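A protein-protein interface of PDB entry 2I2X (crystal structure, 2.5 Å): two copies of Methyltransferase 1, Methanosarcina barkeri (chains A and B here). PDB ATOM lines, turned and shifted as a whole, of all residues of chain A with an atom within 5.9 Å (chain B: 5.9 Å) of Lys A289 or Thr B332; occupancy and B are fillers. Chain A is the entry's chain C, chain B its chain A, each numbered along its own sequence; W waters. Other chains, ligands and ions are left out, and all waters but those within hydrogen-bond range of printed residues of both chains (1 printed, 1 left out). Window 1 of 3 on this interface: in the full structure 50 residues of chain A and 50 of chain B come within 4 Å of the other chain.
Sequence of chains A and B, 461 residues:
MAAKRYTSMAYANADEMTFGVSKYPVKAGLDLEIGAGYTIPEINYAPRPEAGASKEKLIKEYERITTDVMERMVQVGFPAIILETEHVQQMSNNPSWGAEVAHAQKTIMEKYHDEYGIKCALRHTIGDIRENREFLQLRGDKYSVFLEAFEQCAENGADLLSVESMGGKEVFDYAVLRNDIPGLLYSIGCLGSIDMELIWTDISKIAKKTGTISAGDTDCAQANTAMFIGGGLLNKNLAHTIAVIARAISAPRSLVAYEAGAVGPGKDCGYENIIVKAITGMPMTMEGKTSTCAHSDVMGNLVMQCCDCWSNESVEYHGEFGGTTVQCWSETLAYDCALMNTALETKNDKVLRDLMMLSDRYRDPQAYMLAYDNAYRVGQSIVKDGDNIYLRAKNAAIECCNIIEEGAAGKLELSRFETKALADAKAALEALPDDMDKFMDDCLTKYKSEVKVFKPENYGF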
ATOM      1  N   GLU A 287      -4.011  -5.798  31.679  1.00  0.00           N
ATOM      2  CA  GLU A 287      -2.590  -5.572  31.562  1.00  0.00           C
ATOM      3  C   GLU A 287      -2.276  -4.978  30.205  1.00  0.00           C
ATOM      4  O   GLU A 287      -2.970  -5.271  29.248  1.00  0.00           O
ATOM      5  CB  GLU A 287      -1.831  -6.888  31.725  1.00  0.00           C
ATOM      6  CG  GLU A 287      -2.154  -7.970  30.682  1.00  0.00           C
ATOM      7  CD  GLU A 287      -1.482  -9.273  31.033  1.00  0.00           C
ATOM      8  OE1 GLU A 287      -1.634  -9.713  32.185  1.00  0.00           O
ATOM      9  OE2 GLU A 287      -0.785  -9.854  30.183  1.00  0.00           O
ATOM     10  N   GLY A 288      -1.210  -4.190  30.118  1.00  0.00           N
ATOM     11  CA  GLY A 288      -0.838  -3.522  28.882  1.00  0.00           C
ATOM     12  C   GLY A 288       0.537  -2.892  28.977  1.00  0.00           C
ATOM     13  O   GLY A 288       1.531  -3.593  29.166  1.00  0.00           O
ATOM     14  N   LYS A 289       0.604  -1.566  28.891  1.00  0.00           N
ATOM     15  CA  LYS A 289       1.905  -0.894  28.785  1.00  0.00           C
ATOM     16  C   LYS A 289       2.850  -1.153  29.980  1.00  0.00           C
ATOM     17  O   LYS A 289       4.057  -0.955  29.869  1.00  0.00           O
ATOM     18  CB  LYS A 289       1.693   0.601  28.581  1.00  0.00           C
ATOM     19  CG  LYS A 289       1.366   1.345  29.875  1.00  0.00           C
ATOM     20  CD  LYS A 289       1.113   2.779  29.587  1.00  0.00           C
ATOM     21  CE  LYS A 289       0.796   3.629  30.837  1.00  0.00           C
ATOM     22  NZ  LYS A 289       0.524   5.076  30.325  1.00  0.00           N
ATOM     23  N   THR A 290       2.313  -1.564  31.128  1.00  0.00           N
ATOM     24  CA  THR A 290       3.156  -1.760  32.308  1.00  0.00           C
ATOM     25  C   THR A 290       3.297  -3.268  32.613  1.00  0.00           C
ATOM     26  O   THR A 290       3.572  -3.701  33.746  1.00  0.00           O
ATOM     27  CB  THR A 290       2.672  -0.929  33.528  1.00  0.00           C
ATOM     28  OG1 THR A 290       2.480   0.424  33.129  1.00  0.00           O
ATOM     29  CG2 THR A 290       3.708  -0.934  34.623  1.00  0.00           C
ATOM     30  N   SER A 291       3.126  -4.069  31.568  1.00  0.00           N
ATOM     31  CA  SER A 291       3.381  -5.484  31.687  1.00  0.00           C
ATOM     32  C   SER A 291       4.401  -5.906  30.654  1.00  0.00           C
ATOM     33  O   SER A 291       4.536  -7.101  30.389  1.00  0.00           O
ATOM     34  CB  SER A 291       2.084  -6.301  31.553  1.00  0.00           C
ATOM     35  OG  SER A 291       1.485  -6.186  30.261  1.00  0.00           O
ATOM     36  N   THR A 292       5.126  -4.939  30.084  1.00  0.00           N
ATOM     37  CA  THR A 292       6.158  -5.226  29.048  1.00  0.00           C
ATOM     38  C   THR A 292       7.301  -6.112  29.562  1.00  0.00           C
ATOM     39  O   THR A 292       8.019  -6.772  28.780  1.00  0.00           O
ATOM     40  CB  THR A 292       6.737  -3.942  28.492  1.00  0.00           C
ATOM     41  OG1 THR A 292       7.114  -3.087  29.586  1.00  0.00           O
ATOM     42  CG2 THR A 292       5.679  -3.257  27.638  1.00  0.00           C
ATOM     43  N   ASP A 297       2.676  -5.889  23.651  1.00  0.00           N
ATOM     44  CA  ASP A 297       1.363  -5.895  23.046  1.00  0.00           C
ATOM     45  C   ASP A 297       1.069  -4.604  22.318  1.00  0.00           C
ATOM     46  O   ASP A 297       1.858  -3.636  22.330  1.00  0.00           O
ATOM     47  CB  ASP A 297       0.244  -6.292  24.029  1.00  0.00           C
ATOM     48  CG  ASP A 297      -0.109  -5.193  25.034  1.00  0.00           C
ATOM     49  OD1 ASP A 297      -0.440  -4.054  24.605  1.00  0.00           O
ATOM     50  OD2 ASP A 297      -0.126  -5.506  26.261  1.00  0.00           O
ATOM     51  N   MET A 299      -1.909  -2.876  22.502  1.00  0.00           N
ATOM     52  CA  MET A 299      -3.005  -2.154  23.152  1.00  0.00           C
ATOM     53  C   MET A 299      -2.637  -1.630  24.548  1.00  0.00           C
ATOM     54  O   MET A 299      -3.457  -1.666  25.503  1.00  0.00           O
ATOM     55  CB  MET A 299      -4.299  -2.992  23.215  1.00  0.00           C
ATOM     56  CG  MET A 299      -4.184  -4.386  23.816  1.00  0.00           C
ATOM     57  SD  MET A 299      -3.650  -5.547  22.544  1.00  0.00           S
ATOM     58  CE  MET A 299      -5.119  -6.577  22.358  1.00  0.00           C
ATOM     59  N   GLY A 300      -1.413  -1.109  24.649  1.00  0.00           N
ATOM     60  CA  GLY A 300      -0.829  -0.719  25.924  1.00  0.00           C
ATOM     61  C   GLY A 300      -1.651   0.208  26.779  1.00  0.00           C
ATOM     62  O   GLY A 300      -1.744  -0.003  27.963  1.00  0.00           O
ATOM     63  N   ASN A 301      -2.225   1.254  26.199  1.00  0.00           N
ATOM     64  CA  ASN A 301      -3.007   2.208  26.965  1.00  0.00           C
ATOM     65  C   ASN A 301      -4.477   1.865  26.963  1.00  0.00           C
ATOM     66  O   ASN A 301      -5.154   2.008  27.994  1.00  0.00           O
ATOM     67  CB  ASN A 301      -2.863   3.646  26.430  1.00  0.00           C
ATOM     68  CG  ASN A 301      -1.474   4.252  26.664  1.00  0.00           C
ATOM     69  OD1 ASN A 301      -0.874   4.821  25.744  1.00  0.00           O
ATOM     70  ND2 ASN A 301      -0.974   4.137  27.877  1.00  0.00           N
ATOM     71  N   VAL A 303      -6.232  -0.784  27.149  1.00  0.00           N
ATOM     72  CA  VAL A 303      -6.752  -1.773  28.110  1.00  0.00           C
ATOM     73  C   VAL A 303      -7.091  -1.201  29.504  1.00  0.00           C
ATOM     74  O   VAL A 303      -7.870  -1.808  30.269  1.00  0.00           O
ATOM     75  CB  VAL A 303      -5.785  -2.959  28.280  1.00  0.00           C
ATOM     76  CG1 VAL A 303      -5.757  -3.850  26.999  1.00  0.00           C
ATOM     77  CG2 VAL A 303      -4.372  -2.444  28.659  1.00  0.00           C
ATOM     78  N   MET A 304      -6.489  -0.051  29.826  1.00  0.00           N
ATOM     79  CA  MET A 304      -6.753   0.703  31.056  1.00  0.00           C
ATOM     80  C   MET A 304      -8.176   1.326  31.057  1.00  0.00           C
ATOM     81  O   MET A 304      -8.742   1.609  32.124  1.00  0.00           O
ATOM     82  CB  MET A 304      -5.715   1.839  31.224  1.00  0.00           C
ATOM     83  CG  MET A 304      -4.291   1.406  31.547  1.00  0.00           C
ATOM     84  SD  MET A 304      -3.162   2.709  32.157  1.00  0.00           S
ATOM     85  CE  MET A 304      -2.642   3.355  30.612  1.00  0.00           C
ATOM     86  N   TRP A 310      -4.806  -3.329  37.737  1.00  0.00           N
ATOM     87  CA  TRP A 310      -3.822  -3.050  36.721  1.00  0.00           C
ATOM     88  C   TRP A 310      -2.555  -3.837  37.025  1.00  0.00           C
ATOM     89  O   TRP A 310      -1.910  -3.629  38.067  1.00  0.00           O
ATOM     90  CB  TRP A 310      -3.555  -1.552  36.708  1.00  0.00           C
ATOM     91  CG  TRP A 310      -2.614  -1.020  35.639  1.00  0.00           C
ATOM     92  CD1 TRP A 310      -1.544  -0.180  35.832  1.00  0.00           C
ATOM     93  CD2 TRP A 310      -2.705  -1.223  34.234  1.00  0.00           C
ATOM     94  NE1 TRP A 310      -0.956   0.130  34.630  1.00  0.00           N
ATOM     95  CE2 TRP A 310      -1.647  -0.506  33.634  1.00  0.00           C
ATOM     96  CE3 TRP A 310      -3.573  -1.954  33.415  1.00  0.00           C
ATOM     97  CZ2 TRP A 310      -1.447  -0.490  32.248  1.00  0.00           C
ATOM     98  CZ3 TRP A 310      -3.358  -1.956  32.042  1.00  0.00           C
ATOM     99  CH2 TRP A 310      -2.311  -1.225  31.471  1.00  0.00           C
ATOM    100  N   TRP A 329       8.289  -2.563  39.269  1.00  0.00           N
ATOM    101  CA  TRP A 329       7.002  -2.624  38.549  1.00  0.00           C
ATOM    102  C   TRP A 329       5.776  -2.297  39.413  1.00  0.00           C
ATOM    103  O   TRP A 329       4.789  -1.739  38.899  1.00  0.00           O
ATOM    104  CB  TRP A 329       6.821  -3.943  37.786  1.00  0.00           C
ATOM    105  CG  TRP A 329       7.842  -4.131  36.731  1.00  0.00           C
ATOM    106  CD1 TRP A 329       9.029  -4.759  36.870  1.00  0.00           C
ATOM    107  CD2 TRP A 329       7.799  -3.651  35.379  1.00  0.00           C
ATOM    108  NE1 TRP A 329       9.735  -4.723  35.691  1.00  0.00           N
ATOM    109  CE2 TRP A 329       9.001  -4.041  34.762  1.00  0.00           C
ATOM    110  CE3 TRP A 329       6.871  -2.922  34.643  1.00  0.00           C
ATOM    111  CZ2 TRP A 329       9.305  -3.723  33.446  1.00  0.00           C
ATOM    112  CZ3 TRP A 329       7.150  -2.611  33.335  1.00  0.00           C
ATOM    113  CH2 TRP A 329       8.355  -3.013  32.737  1.00  0.00           C
ATOM    114  N   THR A 332       5.437   1.434  39.393  1.00  0.00           N
ATOM    115  CA  THR A 332       4.832   1.947  38.141  1.00  0.00           C
ATOM    116  C   THR A 332       3.315   1.638  38.045  1.00  0.00           C
ATOM    117  O   THR A 332       2.537   2.496  37.624  1.00  0.00           O
ATOM    118  CB  THR A 332       5.601   1.439  36.879  1.00  0.00           C
ATOM    119  OG1 THR A 332       7.006   1.663  37.049  1.00  0.00           O
ATOM    120  CG2 THR A 332       5.142   2.144  35.648  1.00  0.00           C
ATOM    121  N   ASP A 336       0.294   4.439  37.865  1.00  0.00           N
ATOM    122  CA  ASP A 336      -0.720   4.444  36.794  1.00  0.00           C
ATOM    123  C   ASP A 336      -2.109   4.483  37.425  1.00  0.00           C
ATOM    124  O   ASP A 336      -2.998   5.190  36.938  1.00  0.00           O
ATOM    125  CB  ASP A 336      -0.642   3.216  35.899  1.00  0.00           C
ATOM    126  CG  ASP A 336       0.634   3.134  35.080  1.00  0.00           C
ATOM    127  OD1 ASP A 336       1.291   4.156  34.803  1.00  0.00           O
ATOM    128  OD2 ASP A 336       0.979   1.997  34.694  1.00  0.00           O
ATOM    129  N   LYS B 289       7.584   7.854  37.031  1.00  0.00           N
ATOM    130  CA  LYS B 289       7.002   6.530  37.226  1.00  0.00           C
ATOM    131  C   LYS B 289       7.613   5.424  36.346  1.00  0.00           C
ATOM    132  O   LYS B 289       7.596   4.254  36.752  1.00  0.00           O
ATOM    133  CB  LYS B 289       5.487   6.585  37.039  1.00  0.00           C
ATOM    134  CG  LYS B 289       5.024   6.650  35.610  1.00  0.00           C
ATOM    135  CD  LYS B 289       3.572   6.311  35.550  1.00  0.00           C
ATOM    136  CE  LYS B 289       2.896   6.856  34.311  1.00  0.00           C
ATOM    137  NZ  LYS B 289       1.395   6.750  34.471  1.00  0.00           N
ATOM    138  N   THR B 290       8.099   5.791  35.153  1.00  0.00           N
ATOM    139  CA  THR B 290       8.667   4.849  34.210  1.00  0.00           C
ATOM    140  C   THR B 290      10.209   4.883  34.211  1.00  0.00           C
ATOM    141  O   THR B 290      10.871   4.458  33.245  1.00  0.00           O
ATOM    142  CB  THR B 290       8.080   5.018  32.804  1.00  0.00           C
ATOM    143  OG1 THR B 290       6.657   5.069  32.900  1.00  0.00           O
ATOM    144  CG2 THR B 290       8.447   3.807  31.891  1.00  0.00           C
ATOM    145  N   TRP B 310      10.652  11.786  27.665  1.00  0.00           N
ATOM    146  CA  TRP B 310      10.245  10.989  28.819  1.00  0.00           C
ATOM    147  C   TRP B 310      11.172   9.801  28.875  1.00  0.00           C
ATOM    148  O   TRP B 310      11.245   9.015  27.917  1.00  0.00           O
ATOM    149  CB  TRP B 310       8.804  10.568  28.643  1.00  0.00           C
ATOM    150  CG  TRP B 310       8.142   9.783  29.748  1.00  0.00           C
ATOM    151  CD1 TRP B 310       7.441   8.614  29.596  1.00  0.00           C
ATOM    152  CD2 TRP B 310       8.052  10.127  31.137  1.00  0.00           C
ATOM    153  NE1 TRP B 310       6.936   8.199  30.803  1.00  0.00           N
ATOM    154  CE2 TRP B 310       7.282   9.112  31.768  1.00  0.00           C
ATOM    155  CE3 TRP B 310       8.542  11.188  31.913  1.00  0.00           C
ATOM    156  CZ2 TRP B 310       6.991   9.123  33.147  1.00  0.00           C
ATOM    157  CZ3 TRP B 310       8.250  11.206  33.286  1.00  0.00           C
ATOM    158  CH2 TRP B 310       7.480  10.171  33.888  1.00  0.00           C
ATOM    159  N   GLN B 327      14.004  -3.026  25.588  1.00  0.00           N
ATOM    160  CA  GLN B 327      12.727  -3.179  24.903  1.00  0.00           C
ATOM    161  C   GLN B 327      11.548  -3.021  25.829  1.00  0.00           C
ATOM    162  O   GLN B 327      10.619  -2.316  25.502  1.00  0.00           O
ATOM    163  CB  GLN B 327      12.662  -4.509  24.171  1.00  0.00           C
ATOM    164  CG  GLN B 327      13.598  -4.583  22.990  1.00  0.00           C
ATOM    165  CD  GLN B 327      13.706  -5.993  22.464  1.00  0.00           C
ATOM    166  OE1 GLN B 327      13.636  -6.953  23.244  1.00  0.00           O
ATOM    167  NE2 GLN B 327      13.903  -6.133  21.141  1.00  0.00           N
ATOM    168  N   CYS B 328      11.563  -3.654  26.987  1.00  0.00           N
ATOM    169  CA  CYS B 328      10.417  -3.530  27.878  1.00  0.00           C
ATOM    170  C   CYS B 328      10.199  -2.064  28.259  1.00  0.00           C
ATOM    171  O   CYS B 328       9.093  -1.556  28.140  1.00  0.00           O
ATOM    172  CB  CYS B 328      10.623  -4.348  29.148  1.00  0.00           C
ATOM    173  SG  CYS B 328      11.191  -6.027  28.875  1.00  0.00           S
ATOM    174  N   TRP B 329      11.271  -1.377  28.694  1.00  0.00           N
ATOM    175  CA  TRP B 329      11.131  -0.015  29.177  1.00  0.00           C
ATOM    176  C   TRP B 329      10.880   0.972  28.053  1.00  0.00           C
ATOM    177  O   TRP B 329      10.116   1.919  28.258  1.00  0.00           O
ATOM    178  CB  TRP B 329      12.282   0.405  30.070  1.00  0.00           C
ATOM    179  CG  TRP B 329      12.293  -0.319  31.373  1.00  0.00           C
ATOM    180  CD1 TRP B 329      13.021  -1.455  31.688  1.00  0.00           C
ATOM    181  CD2 TRP B 329      11.534   0.003  32.538  1.00  0.00           C
ATOM    182  NE1 TRP B 329      12.755  -1.835  32.980  1.00  0.00           N
ATOM    183  CE2 TRP B 329      11.850  -0.961  33.523  1.00  0.00           C
ATOM    184  CE3 TRP B 329      10.610   0.997  32.838  1.00  0.00           C
ATOM    185  CZ2 TRP B 329      11.275  -0.956  34.787  1.00  0.00           C
ATOM    186  CZ3 TRP B 329      10.033   1.018  34.114  1.00  0.00           C
ATOM    187  CH2 TRP B 329      10.369   0.038  35.073  1.00  0.00           C
ATOM    188  N   SER B 330      11.437   0.744  26.865  1.00  0.00           N
ATOM    189  CA  SER B 330      11.119   1.648  25.752  1.00  0.00           C
ATOM    190  C   SER B 330       9.655   1.576  25.368  1.00  0.00           C
ATOM    191  O   SER B 330       9.035   2.603  25.068  1.00  0.00           O
ATOM    192  CB  SER B 330      12.039   1.472  24.519  1.00  0.00           C
ATOM    193  OG  SER B 330      12.110   0.119  24.084  1.00  0.00           O
ATOM    194  N   GLU B 331       9.091   0.371  25.387  1.00  0.00           N
ATOM    195  CA  GLU B 331       7.667   0.196  25.075  1.00  0.00           C
ATOM    196  C   GLU B 331       6.756   0.963  26.067  1.00  0.00           C
ATOM    197  O   GLU B 331       5.844   1.677  25.634  1.00  0.00           O
ATOM    198  CB  GLU B 331       7.285  -1.299  24.933  1.00  0.00           C
ATOM    199  CG  GLU B 331       5.733  -1.583  24.811  1.00  0.00           C
ATOM    200  CD  GLU B 331       5.366  -2.940  24.213  1.00  0.00           C
ATOM    201  OE1 GLU B 331       6.193  -3.528  23.477  1.00  0.00           O
ATOM    202  OE2 GLU B 331       4.235  -3.431  24.470  1.00  0.00           O
ATOM    203  N   THR B 332       7.017   0.850  27.370  1.00  0.00           N
ATOM    204  CA  THR B 332       6.277   1.625  28.376  1.00  0.00           C
ATOM    205  C   THR B 332       6.443   3.160  28.157  1.00  0.00           C
ATOM    206  O   THR B 332       5.458   3.916  28.135  1.00  0.00           O
ATOM    207  CB  THR B 332       6.692   1.204  29.801  1.00  0.00           C
ATOM    208  OG1 THR B 332       6.745  -0.234  29.905  1.00  0.00           O
ATOM    209  CG2 THR B 332       5.733   1.721  30.801  1.00  0.00           C
ATOM    210  N   LEU B 333       7.679   3.619  27.961  1.00  0.00           N
ATOM    211  CA  LEU B 333       7.904   5.027  27.693  1.00  0.00           C
ATOM    212  C   LEU B 333       7.120   5.480  26.476  1.00  0.00           C
ATOM    213  O   LEU B 333       6.390   6.485  26.524  1.00  0.00           O
ATOM    214  CB  LEU B 333       9.399   5.333  27.457  1.00  0.00           C
ATOM    215  CG  LEU B 333      10.365   5.109  28.610  1.00  0.00           C
ATOM    216  CD1 LEU B 333      11.737   5.128  28.121  1.00  0.00           C
ATOM    217  CD2 LEU B 333      10.163   6.126  29.752  1.00  0.00           C
ATOM    218  N   ALA B 334       7.245   4.734  25.385  1.00  0.00           N
ATOM    219  CA  ALA B 334       6.579   5.143  24.157  1.00  0.00           C
ATOM    220  C   ALA B 334       5.058   5.170  24.318  1.00  0.00           C
ATOM    221  O   ALA B 334       4.374   6.009  23.723  1.00  0.00           O
ATOM    222  CB  ALA B 334       6.982   4.261  23.001  1.00  0.00           C
ATOM    223  N   TYR B 335       4.527   4.265  25.129  1.00  0.00           N
ATOM    224  CA  TYR B 335       3.101   4.267  25.350  1.00  0.00           C
ATOM    225  C   TYR B 335       2.691   5.462  26.216  1.00  0.00           C
ATOM    226  O   TYR B 335       1.658   6.083  25.974  1.00  0.00           O
ATOM    227  CB  TYR B 335       2.667   2.941  25.983  1.00  0.00           C
ATOM    228  CG  TYR B 335       2.202   1.872  25.011  1.00  0.00           C
ATOM    229  CD1 TYR B 335       1.141   2.113  24.127  1.00  0.00           C
ATOM    230  CD2 TYR B 335       2.789   0.611  25.000  1.00  0.00           C
ATOM    231  CE1 TYR B 335       0.687   1.141  23.249  1.00  0.00           C
ATOM    232  CE2 TYR B 335       2.346  -0.373  24.117  1.00  0.00           C
ATOM    233  CZ  TYR B 335       1.297  -0.103  23.233  1.00  0.00           C
ATOM    234  OH  TYR B 335       0.823  -1.102  22.379  1.00  0.00           O
ATOM    235  N   ASP B 336       3.503   5.783  27.233  1.00  0.00           N
ATOM    236  CA  ASP B 336       3.260   6.970  28.064  1.00  0.00           C
ATOM    237  C   ASP B 336       3.220   8.169  27.140  1.00  0.00           C
ATOM    238  O   ASP B 336       2.364   9.030  27.291  1.00  0.00           O
ATOM    239  CB  ASP B 336       4.350   7.178  29.131  1.00  0.00           C
ATOM    240  CG  ASP B 336       4.277   6.170  30.255  1.00  0.00           C
ATOM    241  OD1 ASP B 336       3.189   5.629  30.497  1.00  0.00           O
ATOM    242  OD2 ASP B 336       5.316   5.891  30.891  1.00  0.00           O
ATOM    243  N   CYS B 337       4.138   8.215  26.172  1.00  0.00           N
ATOM    244  CA  CYS B 337       4.130   9.306  25.215  1.00  0.00           C
ATOM    245  C   CYS B 337       2.877   9.279  24.354  1.00  0.00           C
ATOM    246  O   CYS B 337       2.300  10.336  24.080  1.00  0.00           O
ATOM    247  CB  CYS B 337       5.410   9.352  24.369  1.00  0.00           C
ATOM    248  SG  CYS B 337       6.944   9.877  25.320  1.00  0.00           S
ATOM    249  N   LEU B 339      -0.150   8.429  24.995  1.00  0.00           N
ATOM    250  CA  LEU B 339      -1.262   8.976  25.775  1.00  0.00           C
ATOM    251  C   LEU B 339      -1.190  10.482  25.744  1.00  0.00           C
ATOM    252  O   LEU B 339      -2.182  11.195  25.459  1.00  0.00           O
ATOM    253  CB  LEU B 339      -1.189   8.473  27.235  1.00  0.00           C
ATOM    254  CG  LEU B 339      -2.351   8.912  28.129  1.00  0.00           C
ATOM    255  CD1 LEU B 339      -3.685   8.296  27.632  1.00  0.00           C
ATOM    256  CD2 LEU B 339      -2.084   8.617  29.635  1.00  0.00           C
HETATM  257  O   HOH W   1       3.099   4.264  32.800  1.00  0.00           O
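Lys A289 touches Thr B332, and with the chains exchanged Thr A332 touches Lys B289. Lys A289 touches Asp B336, and with the chains exchanged Asp A336 touches Lys B289. Trp B329 touches its own counterpart, Trp A329. 6 positions are printed for both chains. Of the 15 pairs that touch across the chains among the printed residues, 5 have their exchanged pair printed and touching as well.
Printed residues of chain A within 4 Å of Thr B332: Lys A289 (2.8 Å) and Thr A292 (2.9 Å). Of the printed residues of chain B, Asp A297 touches Glu B331 and Tyr B335. Printed residues of chain A within 4 Å of Leu B339: Asn A301 (3.8 Å). Of the printed residues of chain A, Lys B289 touches Thr A332 and Asp A336. Ser A291 touches none of the printed residues of chain B. The nearest residue of chain B that does not touch Lys A289 is Leu B339 (4.5 Å). The nearest printed residue of chain A that does not touch Thr B332 is Trp A329 (4.2 Å).
Water W1 lies within hydrogen-bond range of the side-chain carboxylate (OD1) of Asp B336 (2.7 Å), the side-chain carboxylate (OD1) of Asp A336 (2.7 Å) and the side-chain amino group (NZ) of Lys B289 (3.4 Å).
Printed residues of chain A that touch a printed residue of chain B: Lys A289, Thr A292, Asp A297, Met A299, Gly A300, Asn A301, Trp A329, Thr A332 and Asp A336. Hydrophobic or aromatic side chains of chain A that line the printed part of chain B: Trp A329. Printed residues of chain B that touch a printed residue of chain A: Lys B289, Cys B328, Trp B329, Glu B331, Thr B332, Tyr B335, Asp B336 and Leu B339. Among the printed residues, 15 pairs touch across the chains. Among the printed residues, Asp or Glu carboxylates within 4 Å of a Lys or Arg side-chain nitrogen of the other chain: Lys A289 with Asp B336 and Asp A336 with Lys B289.
O of Asp A297 is in hydrogen-bond range of OH of Tyr B335, at 2.7 Å. OG1 of Thr B332 is in hydrogen-bond range of OG1 of Thr A292. N of Asp A297 lies within hydrogen-bond range of OE2 of Glu B331 (3.0 Å). OG1 of Thr A332 is in hydrogen-bond range of O of Lys B289, 2.7 Å away. O of Lys A289 lies within hydrogen-bond range of OG1 of Thr B332 (2.8 Å). The backbone NH (N) of Met A299 is in hydrogen-bond range of the side-chain hydroxyl (OH) of Tyr B335 (3.3 Å). The side-chain hydroxyl (OG1) of Thr A292 sits at hydrogen-bond distance from the backbone carbonyl oxygen (O) of Cys B328. The backbone carbonyl oxygen (O) of Tyr B335 lies close to the side-chain amide oxygen (OD1) of Asn A301 (2.8 Å). The side-chain hydroxyl (OH) of Tyr B335 lies within hydrogen-bond range of the backbone NH (N) of Gly A300 (3.2 Å). The side-chain carboxylate (OD1) of Asp B336 is in salt-bridge range of the side-chain amino group (NZ) of Lys A289 (2.7 Å). The side-chain amino group (NZ) of Lys B289 is in salt-bridge range of the side-chain carboxylate (OD1) of Asp A336, at 2.6 Å.
CB of Tyr B335 touches CB of Lys A289, at 3.6 Å. Thr A292 touches Glu B331. Leu B339 touches Asn A301. CZ2 of Trp A329 touches CZ2 of Trp B329, at 3.7 Å.
The side-chain hydroxyl (OG1) of Thr A290 is in hydrogen-bond range of the side-chain carboxylate (OD2) of Asp A336. The backbone carbonyl oxygen (O) of Cys B328 is in hydrogen-bond range of the side-chain hydroxyl (OG1) of Thr B332 (3.2 Å). The side-chain carboxylate (OD2) of Asp B336 is in hydrogen-bond range of the indole nitrogen (NE1) of Trp B310, 2.8 Å away. OD2 of Asp A336 lies within hydrogen-bond range of NE1 of Trp A310 (2.7 Å). The backbone NH of Gly A300 is in hydrogen-bond range of the side-chain carboxylate of Asp A297. The backbone NH of Lys A289 lies within hydrogen-bond range of the backbone carbonyl oxygen of Gly A300.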
